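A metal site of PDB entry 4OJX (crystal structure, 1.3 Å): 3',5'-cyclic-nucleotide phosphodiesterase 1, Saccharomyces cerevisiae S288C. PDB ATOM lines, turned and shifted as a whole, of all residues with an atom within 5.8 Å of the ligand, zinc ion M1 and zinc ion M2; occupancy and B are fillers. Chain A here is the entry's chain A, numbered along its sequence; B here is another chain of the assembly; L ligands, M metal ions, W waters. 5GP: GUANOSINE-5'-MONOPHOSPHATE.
The backbone carbonyl oxygen of Glu 289 is in hydrogen-bond range of an oxygen (O2') of the ligand (3.4 Å). O1P of the ligand is in salt-bridge range of NZ of Lys 328 (2.8 Å). O1P of the ligand is in hydrogen-bond range of NE2 of His 294.
A ring nitrogen (ND1) of His 294 is in hydrogen-bond range of the side-chain hydroxyl (OG) of Ser 281. N of Lys 328 sits at hydrogen-bond distance from O of Ser 281 (3.0 Å). ND1 of His 326 lies within hydrogen-bond range of OG of Ser 281 (2.9 Å). The side-chain amino group (NZ) of Lys 328 lies within hydrogen-bond range of the backbone carbonyl oxygen (O) of Gly 13, at 2.8 Å.
Merely in contact with the ligand: Pro 176 of chain B (3.2 Å), Tyr 145 of chain B (3.2 Å), Trp 175 of chain B (3.5 Å), Val 217 (3.5 Å), Leu 178 of chain B (3.8 Å), Pro 142 of chain B (3.8 Å), Gly 13 (3.9 Å) and Glu 181 of chain B (3.9 Å). Hydrophobic or aromatic side chains that line the ligand: His 130, His 213, Val 217, His 294, His 326, Pro 142 of chain B, Tyr 145 of chain B, Trp 175 of chain B, Pro 176 of chain B and Leu 178 of chain B. The nearest printed residue that does not touch the ligand is Tyr 292 (4.01 Å).
Water W3 binds zinc ion M1 (2.0 Å). Zinc ion M1 is bound by NE2 of His 213, at 2.1 Å. A ring nitrogen (NE2) of His 128 binds zinc ion M1, at 2.2 Å. Zinc ion M1 is bound by ND1 of His 130, at 2.2 Å. An oxygen (O2P) of the ligand binds zinc ion M1 (2.2 Å). OD2 of Asp 244 is bound to zinc ion M1, at 2.2 Å. Zinc ion M1 has six donor atoms within binding distance.
Zinc ion M2 is bound by water W3 (2.0 Å), a ring nitrogen (NE2) of His 326 (2.1 Å), a ring nitrogen (NE2) of His 133 (2.1 Å), the side-chain carboxylate of Asp 244 (2.1 Å), the side-chain carboxylate of Asp 132 (2.2 Å) and an oxygen (O3P) of the ligand (2.3 Å). Zinc ion M2 has six donor atoms within binding distance.
Water W3 bridges OD1 of Asp 132 (2.7 Å) and O5' of the ligand (3.4 Å). Water W4 lies within hydrogen-bond range of O3' of the ligand (2.4 Å) and NZ of Lys 328 (2.8 Å). Water W2 lies within hydrogen-bond range of O of Ile 215 (2.7 Å) and O6 of the ligand (2.8 Å). Water W1 lies within hydrogen-bond range of the backbone carbonyl oxygen (O) of Gly 13 (2.9 Å) and an oxygen (O5') of the ligand (3.3 Å).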
ATOM      1  N   GLY A  13      13.191 -12.287  10.303  1.00  0.00           N
ATOM      2  CA  GLY A  13      13.667 -13.043   9.151  1.00  0.00           C
ATOM      3  C   GLY A  13      12.654 -13.976   8.518  1.00  0.00           C
ATOM      4  O   GLY A  13      12.956 -14.606   7.514  1.00  0.00           O
ATOM      5  N   GLN A  21      12.221  -7.145   7.099  1.00  0.00           N
ATOM      6  CA  GLN A  21      13.337  -6.206   7.167  1.00  0.00           C
ATOM      7  C   GLN A  21      13.051  -4.808   6.611  1.00  0.00           C
ATOM      8  O   GLN A  21      12.756  -4.646   5.419  1.00  0.00           O
ATOM      9  CB  GLN A  21      14.558  -6.792   6.468  1.00  0.00           C
ATOM     10  CG  GLN A  21      15.777  -5.887   6.582  1.00  0.00           C
ATOM     11  CD  GLN A  21      17.075  -6.657   6.545  1.00  0.00           C
ATOM     12  OE1 GLN A  21      17.308  -7.542   7.361  1.00  0.00           O
ATOM     13  NE2 GLN A  21      17.944  -6.303   5.609  1.00  0.00           N
ATOM     14  N   HIS A 128      17.962  -6.690  -1.798  1.00  0.00           N
ATOM     15  CA  HIS A 128      17.636  -7.747  -2.747  1.00  0.00           C
ATOM     16  C   HIS A 128      16.140  -7.847  -2.827  1.00  0.00           C
ATOM     17  O   HIS A 128      15.448  -7.382  -1.917  1.00  0.00           O
ATOM     18  CB  HIS A 128      18.322  -9.068  -2.383  1.00  0.00           C
ATOM     19  CG  HIS A 128      17.782  -9.770  -1.138  1.00  0.00           C
ATOM     20  ND1 HIS A 128      17.860  -9.246   0.106  1.00  0.00           N
ATOM     21  CD2 HIS A 128      17.218 -11.030  -1.001  1.00  0.00           C
ATOM     22  CE1 HIS A 128      17.357 -10.137   0.998  1.00  0.00           C
ATOM     23  NE2 HIS A 128      16.970 -11.233   0.326  1.00  0.00           N
ATOM     24  N   HIS A 130      13.875 -10.295  -2.686  1.00  0.00           N
ATOM     25  CA  HIS A 130      13.019 -11.273  -1.999  1.00  0.00           C
ATOM     26  C   HIS A 130      11.858 -10.565  -1.352  1.00  0.00           C
ATOM     27  O   HIS A 130      12.010  -9.456  -0.810  1.00  0.00           O
ATOM     28  CB  HIS A 130      13.779 -12.048  -0.935  1.00  0.00           C
ATOM     29  CG  HIS A 130      14.594 -13.196  -1.491  1.00  0.00           C
ATOM     30  ND1 HIS A 130      15.604 -13.760  -0.783  1.00  0.00           N
ATOM     31  CD2 HIS A 130      14.496 -13.890  -2.685  1.00  0.00           C
ATOM     32  CE1 HIS A 130      16.129 -14.764  -1.501  1.00  0.00           C
ATOM     33  NE2 HIS A 130      15.454 -14.840  -2.662  1.00  0.00           N
ATOM     34  N   ASP A 132      10.101 -10.583   1.323  1.00  0.00           N
ATOM     35  CA  ASP A 132      10.162 -10.070   2.702  1.00  0.00           C
ATOM     36  C   ASP A 132      10.885  -8.731   2.803  1.00  0.00           C
ATOM     37  O   ASP A 132      10.728  -8.025   3.809  1.00  0.00           O
ATOM     38  CB  ASP A 132      10.726 -11.090   3.721  1.00  0.00           C
ATOM     39  CG  ASP A 132      12.127 -11.603   3.363  1.00  0.00           C
ATOM     40  OD1 ASP A 132      12.273 -12.012   2.187  1.00  0.00           O
ATOM     41  OD2 ASP A 132      13.087 -11.613   4.229  1.00  0.00           O
ATOM     42  N   HIS A 133      11.657  -8.359   1.774  1.00  0.00           N
ATOM     43  CA  HIS A 133      12.404  -7.099   1.771  1.00  0.00           C
ATOM     44  C   HIS A 133      11.735  -6.028   0.977  1.00  0.00           C
ATOM     45  O   HIS A 133      12.260  -4.917   0.913  1.00  0.00           O
ATOM     46  CB  HIS A 133      13.852  -7.315   1.322  1.00  0.00           C
ATOM     47  CG  HIS A 133      14.599  -8.229   2.242  1.00  0.00           C
ATOM     48  ND1 HIS A 133      15.552  -7.811   3.113  1.00  0.00           N
ATOM     49  CD2 HIS A 133      14.442  -9.576   2.456  1.00  0.00           C
ATOM     50  CE1 HIS A 133      15.960  -8.862   3.842  1.00  0.00           C
ATOM     51  NE2 HIS A 133      15.273  -9.930   3.452  1.00  0.00           N
ATOM     52  N   HIS A 213      23.986 -14.713  -1.475  1.00  0.00           N
ATOM     53  CA  HIS A 213      22.809 -15.045  -0.670  1.00  0.00           C
ATOM     54  C   HIS A 213      22.179 -16.322  -1.181  1.00  0.00           C
ATOM     55  O   HIS A 213      20.982 -16.418  -1.402  1.00  0.00           O
ATOM     56  CB  HIS A 213      21.872 -13.842  -0.676  1.00  0.00           C
ATOM     57  CG  HIS A 213      20.542 -14.043   0.028  1.00  0.00           C
ATOM     58  ND1 HIS A 213      20.384 -14.836   1.099  1.00  0.00           N
ATOM     59  CD2 HIS A 213      19.286 -13.489  -0.238  1.00  0.00           C
ATOM     60  CE1 HIS A 213      19.094 -14.830   1.486  1.00  0.00           C
ATOM     61  NE2 HIS A 213      18.427 -13.993   0.678  1.00  0.00           N
ATOM     62  N   ILE A 215      21.614 -19.901  -3.546  1.00  0.00           N
ATOM     63  CA  ILE A 215      21.458 -20.283  -4.946  1.00  0.00           C
ATOM     64  C   ILE A 215      19.997 -20.570  -5.243  1.00  0.00           C
ATOM     65  O   ILE A 215      19.220 -20.921  -4.347  1.00  0.00           O
ATOM     66  CB  ILE A 215      22.336 -21.511  -5.331  1.00  0.00           C
ATOM     67  CG1 ILE A 215      21.991 -22.727  -4.456  1.00  0.00           C
ATOM     68  CG2 ILE A 215      23.823 -21.166  -5.262  1.00  0.00           C
ATOM     69  CD1 ILE A 215      22.581 -24.038  -4.935  1.00  0.00           C
ATOM     70  N   VAL A 217      16.700 -22.488  -6.232  1.00  0.00           N
ATOM     71  CA  VAL A 217      16.241 -23.862  -6.053  1.00  0.00           C
ATOM     72  C   VAL A 217      16.145 -24.587  -7.388  1.00  0.00           C
ATOM     73  O   VAL A 217      16.654 -25.701  -7.538  1.00  0.00           O
ATOM     74  CB  VAL A 217      14.864 -23.883  -5.346  1.00  0.00           C
ATOM     75  CG1 VAL A 217      14.363 -25.313  -5.188  1.00  0.00           C
ATOM     76  CG2 VAL A 217      14.929 -23.168  -4.006  1.00  0.00           C
ATOM     77  N   ASP A 244      20.510  -9.853   3.341  1.00  0.00           N
ATOM     78  CA  ASP A 244      20.706 -11.273   3.665  1.00  0.00           C
ATOM     79  C   ASP A 244      22.012 -11.733   3.007  1.00  0.00           C
ATOM     80  O   ASP A 244      22.342 -11.279   1.893  1.00  0.00           O
ATOM     81  CB  ASP A 244      19.554 -12.179   3.137  1.00  0.00           C
ATOM     82  CG  ASP A 244      18.123 -11.803   3.642  1.00  0.00           C
ATOM     83  OD1 ASP A 244      18.119 -10.839   4.488  1.00  0.00           O
ATOM     84  OD2 ASP A 244      17.062 -12.447   3.147  1.00  0.00           O
ATOM     85  N   SER A 281      20.449 -15.272  10.865  1.00  0.00           N
ATOM     86  CA  SER A 281      19.102 -15.839  10.741  1.00  0.00           C
ATOM     87  C   SER A 281      18.857 -17.024  11.659  1.00  0.00           C
ATOM     88  O   SER A 281      17.748 -17.212  12.135  1.00  0.00           O
ATOM     89  CB  SER A 281      18.812 -16.276   9.305  1.00  0.00           C
ATOM     90  OG  SER A 281      18.723 -15.182   8.422  1.00  0.00           O
ATOM     91  N   GLU A 289      17.963 -26.610   5.918  1.00  0.00           N
ATOM     92  CA  GLU A 289      16.941 -25.957   5.094  1.00  0.00           C
ATOM     93  C   GLU A 289      16.702 -24.487   5.444  1.00  0.00           C
ATOM     94  O   GLU A 289      16.510 -23.658   4.545  1.00  0.00           O
ATOM     95  CB  GLU A 289      15.612 -26.723   5.164  1.00  0.00           C
ATOM     96  CG  GLU A 289      15.607 -28.080   4.460  1.00  0.00           C
ATOM     97  CD  GLU A 289      16.369 -29.147   5.215  1.00  0.00           C
ATOM     98  OE1 GLU A 289      16.305 -29.170   6.459  1.00  0.00           O
ATOM     99  OE2 GLU A 289      17.037 -29.986   4.555  1.00  0.00           O
ATOM    100  N   GLN A 290      16.722 -24.165   6.736  1.00  0.00           N
ATOM    101  CA  GLN A 290      16.496 -22.800   7.197  1.00  0.00           C
ATOM    102  C   GLN A 290      17.747 -21.916   7.038  1.00  0.00           C
ATOM    103  O   GLN A 290      17.634 -20.696   6.915  1.00  0.00           O
ATOM    104  CB  GLN A 290      16.008 -22.780   8.645  1.00  0.00           C
ATOM    105  CG  GLN A 290      15.081 -21.609   8.954  1.00  0.00           C
ATOM    106  CD  GLN A 290      14.718 -21.476  10.434  1.00  0.00           C
ATOM    107  OE1 GLN A 290      15.547 -21.720  11.312  1.00  0.00           O
ATOM    108  NE2 GLN A 290      13.490 -21.064  10.702  1.00  0.00           N
ATOM    109  N   LEU A 291      18.916 -22.552   7.023  1.00  0.00           N
ATOM    110  CA  LEU A 291      20.200 -21.843   6.962  1.00  0.00           C
ATOM    111  C   LEU A 291      20.663 -21.434   5.556  1.00  0.00           C
ATOM    112  O   LEU A 291      21.461 -20.499   5.422  1.00  0.00           O
ATOM    113  CB  LEU A 291      21.300 -22.654   7.682  1.00  0.00           C
ATOM    114  CG  LEU A 291      22.693 -22.040   7.861  1.00  0.00           C
ATOM    115  CD1 LEU A 291      22.631 -20.777   8.725  1.00  0.00           C
ATOM    116  CD2 LEU A 291      23.659 -23.051   8.459  1.00  0.00           C
ATOM    117  N   TYR A 292      20.160 -22.102   4.521  1.00  0.00           N
ATOM    118  CA  TYR A 292      20.544 -21.804   3.127  1.00  0.00           C
ATOM    119  C   TYR A 292      20.468 -20.316   2.737  1.00  0.00           C
ATOM    120  O   TYR A 292      19.400 -19.694   2.783  1.00  0.00           O
ATOM    121  CB  TYR A 292      19.738 -22.645   2.130  1.00  0.00           C
ATOM    122  CG  TYR A 292      19.963 -24.148   2.205  1.00  0.00           C
ATOM    123  CD1 TYR A 292      18.902 -25.032   2.035  1.00  0.00           C
ATOM    124  CD2 TYR A 292      21.244 -24.681   2.442  1.00  0.00           C
ATOM    125  CE1 TYR A 292      19.097 -26.404   2.096  1.00  0.00           C
ATOM    126  CE2 TYR A 292      21.438 -26.053   2.502  1.00  0.00           C
ATOM    127  CZ  TYR A 292      20.364 -26.906   2.333  1.00  0.00           C
ATOM    128  OH  TYR A 292      20.553 -28.270   2.390  1.00  0.00           O
ATOM    129  N   HIS A 294      22.147 -17.934   4.310  1.00  0.00           N
ATOM    130  CA  HIS A 294      22.165 -17.118   5.531  1.00  0.00           C
ATOM    131  C   HIS A 294      23.340 -17.414   6.398  1.00  0.00           C
ATOM    132  O   HIS A 294      24.156 -18.297   6.083  1.00  0.00           O
ATOM    133  CB  HIS A 294      20.882 -17.354   6.318  1.00  0.00           C
ATOM    134  CG  HIS A 294      19.653 -16.831   5.644  1.00  0.00           C
ATOM    135  ND1 HIS A 294      19.471 -15.527   5.368  1.00  0.00           N
ATOM    136  CD2 HIS A 294      18.526 -17.492   5.166  1.00  0.00           C
ATOM    137  CE1 HIS A 294      18.303 -15.362   4.752  1.00  0.00           C
ATOM    138  NE2 HIS A 294      17.721 -16.570   4.630  1.00  0.00           N
ATOM    139  N   HIS A 326      17.247  -9.971  11.236  1.00  0.00           N
ATOM    140  CA  HIS A 326      16.734 -11.053  10.390  1.00  0.00           C
ATOM    141  C   HIS A 326      16.736 -12.394  11.079  1.00  0.00           C
ATOM    142  O   HIS A 326      16.901 -13.430  10.428  1.00  0.00           O
ATOM    143  CB  HIS A 326      17.529 -11.079   9.079  1.00  0.00           C
ATOM    144  CG  HIS A 326      16.807 -11.721   7.916  1.00  0.00           C
ATOM    145  ND1 HIS A 326      16.825 -13.051   7.677  1.00  0.00           N
ATOM    146  CD2 HIS A 326      16.085 -11.149   6.873  1.00  0.00           C
ATOM    147  CE1 HIS A 326      16.131 -13.312   6.559  1.00  0.00           C
ATOM    148  NE2 HIS A 326      15.676 -12.156   6.070  1.00  0.00           N
ATOM    149  N   LYS A 328      15.212 -15.633  12.345  1.00  0.00           N
ATOM    150  CA  LYS A 328      14.023 -16.372  11.962  1.00  0.00           C
ATOM    151  C   LYS A 328      13.289 -16.948  13.170  1.00  0.00           C
ATOM    152  O   LYS A 328      13.914 -17.295  14.194  1.00  0.00           O
ATOM    153  CB  LYS A 328      14.419 -17.489  11.000  1.00  0.00           C
ATOM    154  CG  LYS A 328      14.765 -16.946   9.620  1.00  0.00           C
ATOM    155  CD  LYS A 328      15.159 -18.045   8.643  1.00  0.00           C
ATOM    156  CE  LYS A 328      15.490 -17.469   7.272  1.00  0.00           C
ATOM    157  NZ  LYS A 328      14.328 -16.835   6.572  1.00  0.00           N
ATOM    158  N   PRO B 142       8.185 -21.239   3.809  1.00  0.00           N
ATOM    159  CA  PRO B 142       9.273 -22.129   4.268  1.00  0.00           C
ATOM    160  C   PRO B 142       8.924 -22.948   5.514  1.00  0.00           C
ATOM    161  O   PRO B 142       9.622 -23.932   5.790  1.00  0.00           O
ATOM    162  CB  PRO B 142      10.425 -21.161   4.530  1.00  0.00           C
ATOM    163  CG  PRO B 142      10.136 -20.001   3.641  1.00  0.00           C
ATOM    164  CD  PRO B 142       8.647 -19.846   3.701  1.00  0.00           C
ATOM    165  N   TYR B 145       8.847 -26.826   5.562  1.00  0.00           N
ATOM    166  CA  TYR B 145      10.051 -27.647   5.711  1.00  0.00           C
ATOM    167  C   TYR B 145      10.504 -27.916   7.147  1.00  0.00           C
ATOM    168  O   TYR B 145      11.566 -28.514   7.358  1.00  0.00           O
ATOM    169  CB  TYR B 145      11.195 -27.043   4.905  1.00  0.00           C
ATOM    170  CG  TYR B 145      10.857 -26.863   3.455  1.00  0.00           C
ATOM    171  CD1 TYR B 145      10.653 -27.970   2.634  1.00  0.00           C
ATOM    172  CD2 TYR B 145      10.696 -25.599   2.918  1.00  0.00           C
ATOM    173  CE1 TYR B 145      10.325 -27.815   1.297  1.00  0.00           C
ATOM    174  CE2 TYR B 145      10.367 -25.428   1.589  1.00  0.00           C
ATOM    175  CZ  TYR B 145      10.179 -26.542   0.784  1.00  0.00           C
ATOM    176  OH  TYR B 145       9.851 -26.371  -0.545  1.00  0.00           O
ATOM    177  N   TRP B 175      11.234 -15.024  -4.883  1.00  0.00           N
ATOM    178  CA  TRP B 175      11.177 -16.013  -3.828  1.00  0.00           C
ATOM    179  C   TRP B 175      11.860 -17.245  -4.329  1.00  0.00           C
ATOM    180  O   TRP B 175      11.752 -17.553  -5.520  1.00  0.00           O
ATOM    181  CB  TRP B 175       9.742 -16.361  -3.460  1.00  0.00           C
ATOM    182  CG  TRP B 175       9.630 -16.918  -2.077  1.00  0.00           C
ATOM    183  CD1 TRP B 175       9.216 -18.182  -1.696  1.00  0.00           C
ATOM    184  CD2 TRP B 175       9.943 -16.220  -0.835  1.00  0.00           C
ATOM    185  NE1 TRP B 175       9.249 -18.318  -0.328  1.00  0.00           N
ATOM    186  CE2 TRP B 175       9.691 -17.167   0.242  1.00  0.00           C
ATOM    187  CE3 TRP B 175      10.405 -14.953  -0.537  1.00  0.00           C
ATOM    188  CZ2 TRP B 175       9.866 -16.814   1.570  1.00  0.00           C
ATOM    189  CZ3 TRP B 175      10.597 -14.606   0.807  1.00  0.00           C
ATOM    190  CH2 TRP B 175      10.326 -15.524   1.831  1.00  0.00           C
ATOM    191  N   PRO B 176      12.547 -17.990  -3.439  1.00  0.00           N
ATOM    192  CA  PRO B 176      13.038 -19.297  -3.881  1.00  0.00           C
ATOM    193  C   PRO B 176      11.922 -20.127  -4.490  1.00  0.00           C
ATOM    194  O   PRO B 176      10.776 -20.086  -4.007  1.00  0.00           O
ATOM    195  CB  PRO B 176      13.563 -19.915  -2.576  1.00  0.00           C
ATOM    196  CG  PRO B 176      14.010 -18.719  -1.781  1.00  0.00           C
ATOM    197  CD  PRO B 176      12.926 -17.701  -2.043  1.00  0.00           C
ATOM    198  N   LEU B 178      10.093 -22.799  -4.459  1.00  0.00           N
ATOM    199  CA  LEU B 178       9.804 -23.939  -3.605  1.00  0.00           C
ATOM    200  C   LEU B 178       8.989 -24.986  -4.341  1.00  0.00           C
ATOM    201  O   LEU B 178       8.998 -26.147  -3.941  1.00  0.00           O
ATOM    202  CB  LEU B 178       9.109 -23.501  -2.310  1.00  0.00           C
ATOM    203  CG  LEU B 178       9.921 -22.526  -1.455  1.00  0.00           C
ATOM    204  CD1 LEU B 178       9.138 -22.212  -0.190  1.00  0.00           C
ATOM    205  CD2 LEU B 178      11.302 -23.066  -1.105  1.00  0.00           C
ATOM    206  N   GLU B 181      11.306 -27.895  -5.583  1.00  0.00           N
ATOM    207  CA  GLU B 181      11.796 -28.869  -4.605  1.00  0.00           C
ATOM    208  C   GLU B 181      11.147 -30.228  -4.892  1.00  0.00           C
ATOM    209  O   GLU B 181       9.938 -30.314  -5.067  1.00  0.00           O
ATOM    210  CB  GLU B 181      11.480 -28.397  -3.182  1.00  0.00           C
ATOM    211  CG  GLU B 181      11.656 -29.434  -2.075  1.00  0.00           C
ATOM    212  CD  GLU B 181      13.108 -29.628  -1.682  1.00  0.00           C
ATOM    213  OE1 GLU B 181      13.895 -30.154  -2.500  1.00  0.00           O
ATOM    214  OE2 GLU B 181      13.456 -29.257  -0.543  1.00  0.00           O
HETATM  215  P   5GP L   1      15.033 -15.399   3.213  1.00  0.00           P
HETATM  216  O1P 5GP L   1      15.336 -16.597   4.018  1.00  0.00           O
HETATM  217  O2P 5GP L   1      16.054 -15.115   2.144  1.00  0.00           O
HETATM  218  O3P 5GP L   1      14.736 -14.218   4.105  1.00  0.00           O
HETATM  219  O5' 5GP L   1      13.701 -15.819   2.483  1.00  0.00           O
HETATM  220  C5' 5GP L   1      13.733 -16.999   1.615  1.00  0.00           C
HETATM  221  C4' 5GP L   1      13.320 -18.359   2.279  1.00  0.00           C
HETATM  222  O4' 5GP L   1      13.415 -19.429   1.299  1.00  0.00           O
HETATM  223  C3' 5GP L   1      14.285 -18.776   3.388  1.00  0.00           C
HETATM  224  O3' 5GP L   1      13.628 -18.658   4.654  1.00  0.00           O
HETATM  225  C2' 5GP L   1      14.692 -20.224   3.153  1.00  0.00           C
HETATM  226  O2' 5GP L   1      14.309 -21.038   4.283  1.00  0.00           O
HETATM  227  C1' 5GP L   1      13.890 -20.656   1.935  1.00  0.00           C
HETATM  228  N9  5GP L   1      14.738 -21.457   0.989  1.00  0.00           N
HETATM  229  C8  5GP L   1      15.610 -20.914   0.142  1.00  0.00           C
HETATM  230  N7  5GP L   1      16.182 -21.899  -0.556  1.00  0.00           N
HETATM  231  C5  5GP L   1      15.665 -23.044  -0.144  1.00  0.00           C
HETATM  232  C6  5GP L   1      15.906 -24.310  -0.525  1.00  0.00           C
HETATM  233  O6  5GP L   1      16.737 -24.555  -1.400  1.00  0.00           O
HETATM  234  N1  5GP L   1      15.227 -25.365   0.088  1.00  0.00           N
HETATM  235  C2  5GP L   1      14.293 -25.059   1.081  1.00  0.00           C
HETATM  236  N2  5GP L   1      13.633 -26.055   1.667  1.00  0.00           N
HETATM  237  N3  5GP L   1      14.085 -23.781   1.427  1.00  0.00           N
HETATM  238  C4  5GP L   1      14.765 -22.775   0.824  1.00  0.00           C
HETATM  239 ZN    ZN M   1      16.486 -13.191   1.115  1.00  0.00          ZN
HETATM  240 ZN    ZN M   2      15.204 -11.952   4.040  1.00  0.00          ZN
HETATM  241  O   HOH W   1      11.814 -14.639   4.854  1.00  0.00           O
HETATM  242  O   HOH W   2      18.621 -22.907  -2.547  1.00  0.00           O
HETATM  243  O   HOH W   3      14.884 -12.613   2.166  1.00  0.00           O
HETATM  244  O   HOH W   4      12.096 -18.527   6.555  1.00  0.00           O
HETATM  245  O   HOH W   5      17.140 -17.553   1.092  1.00  0.00           O
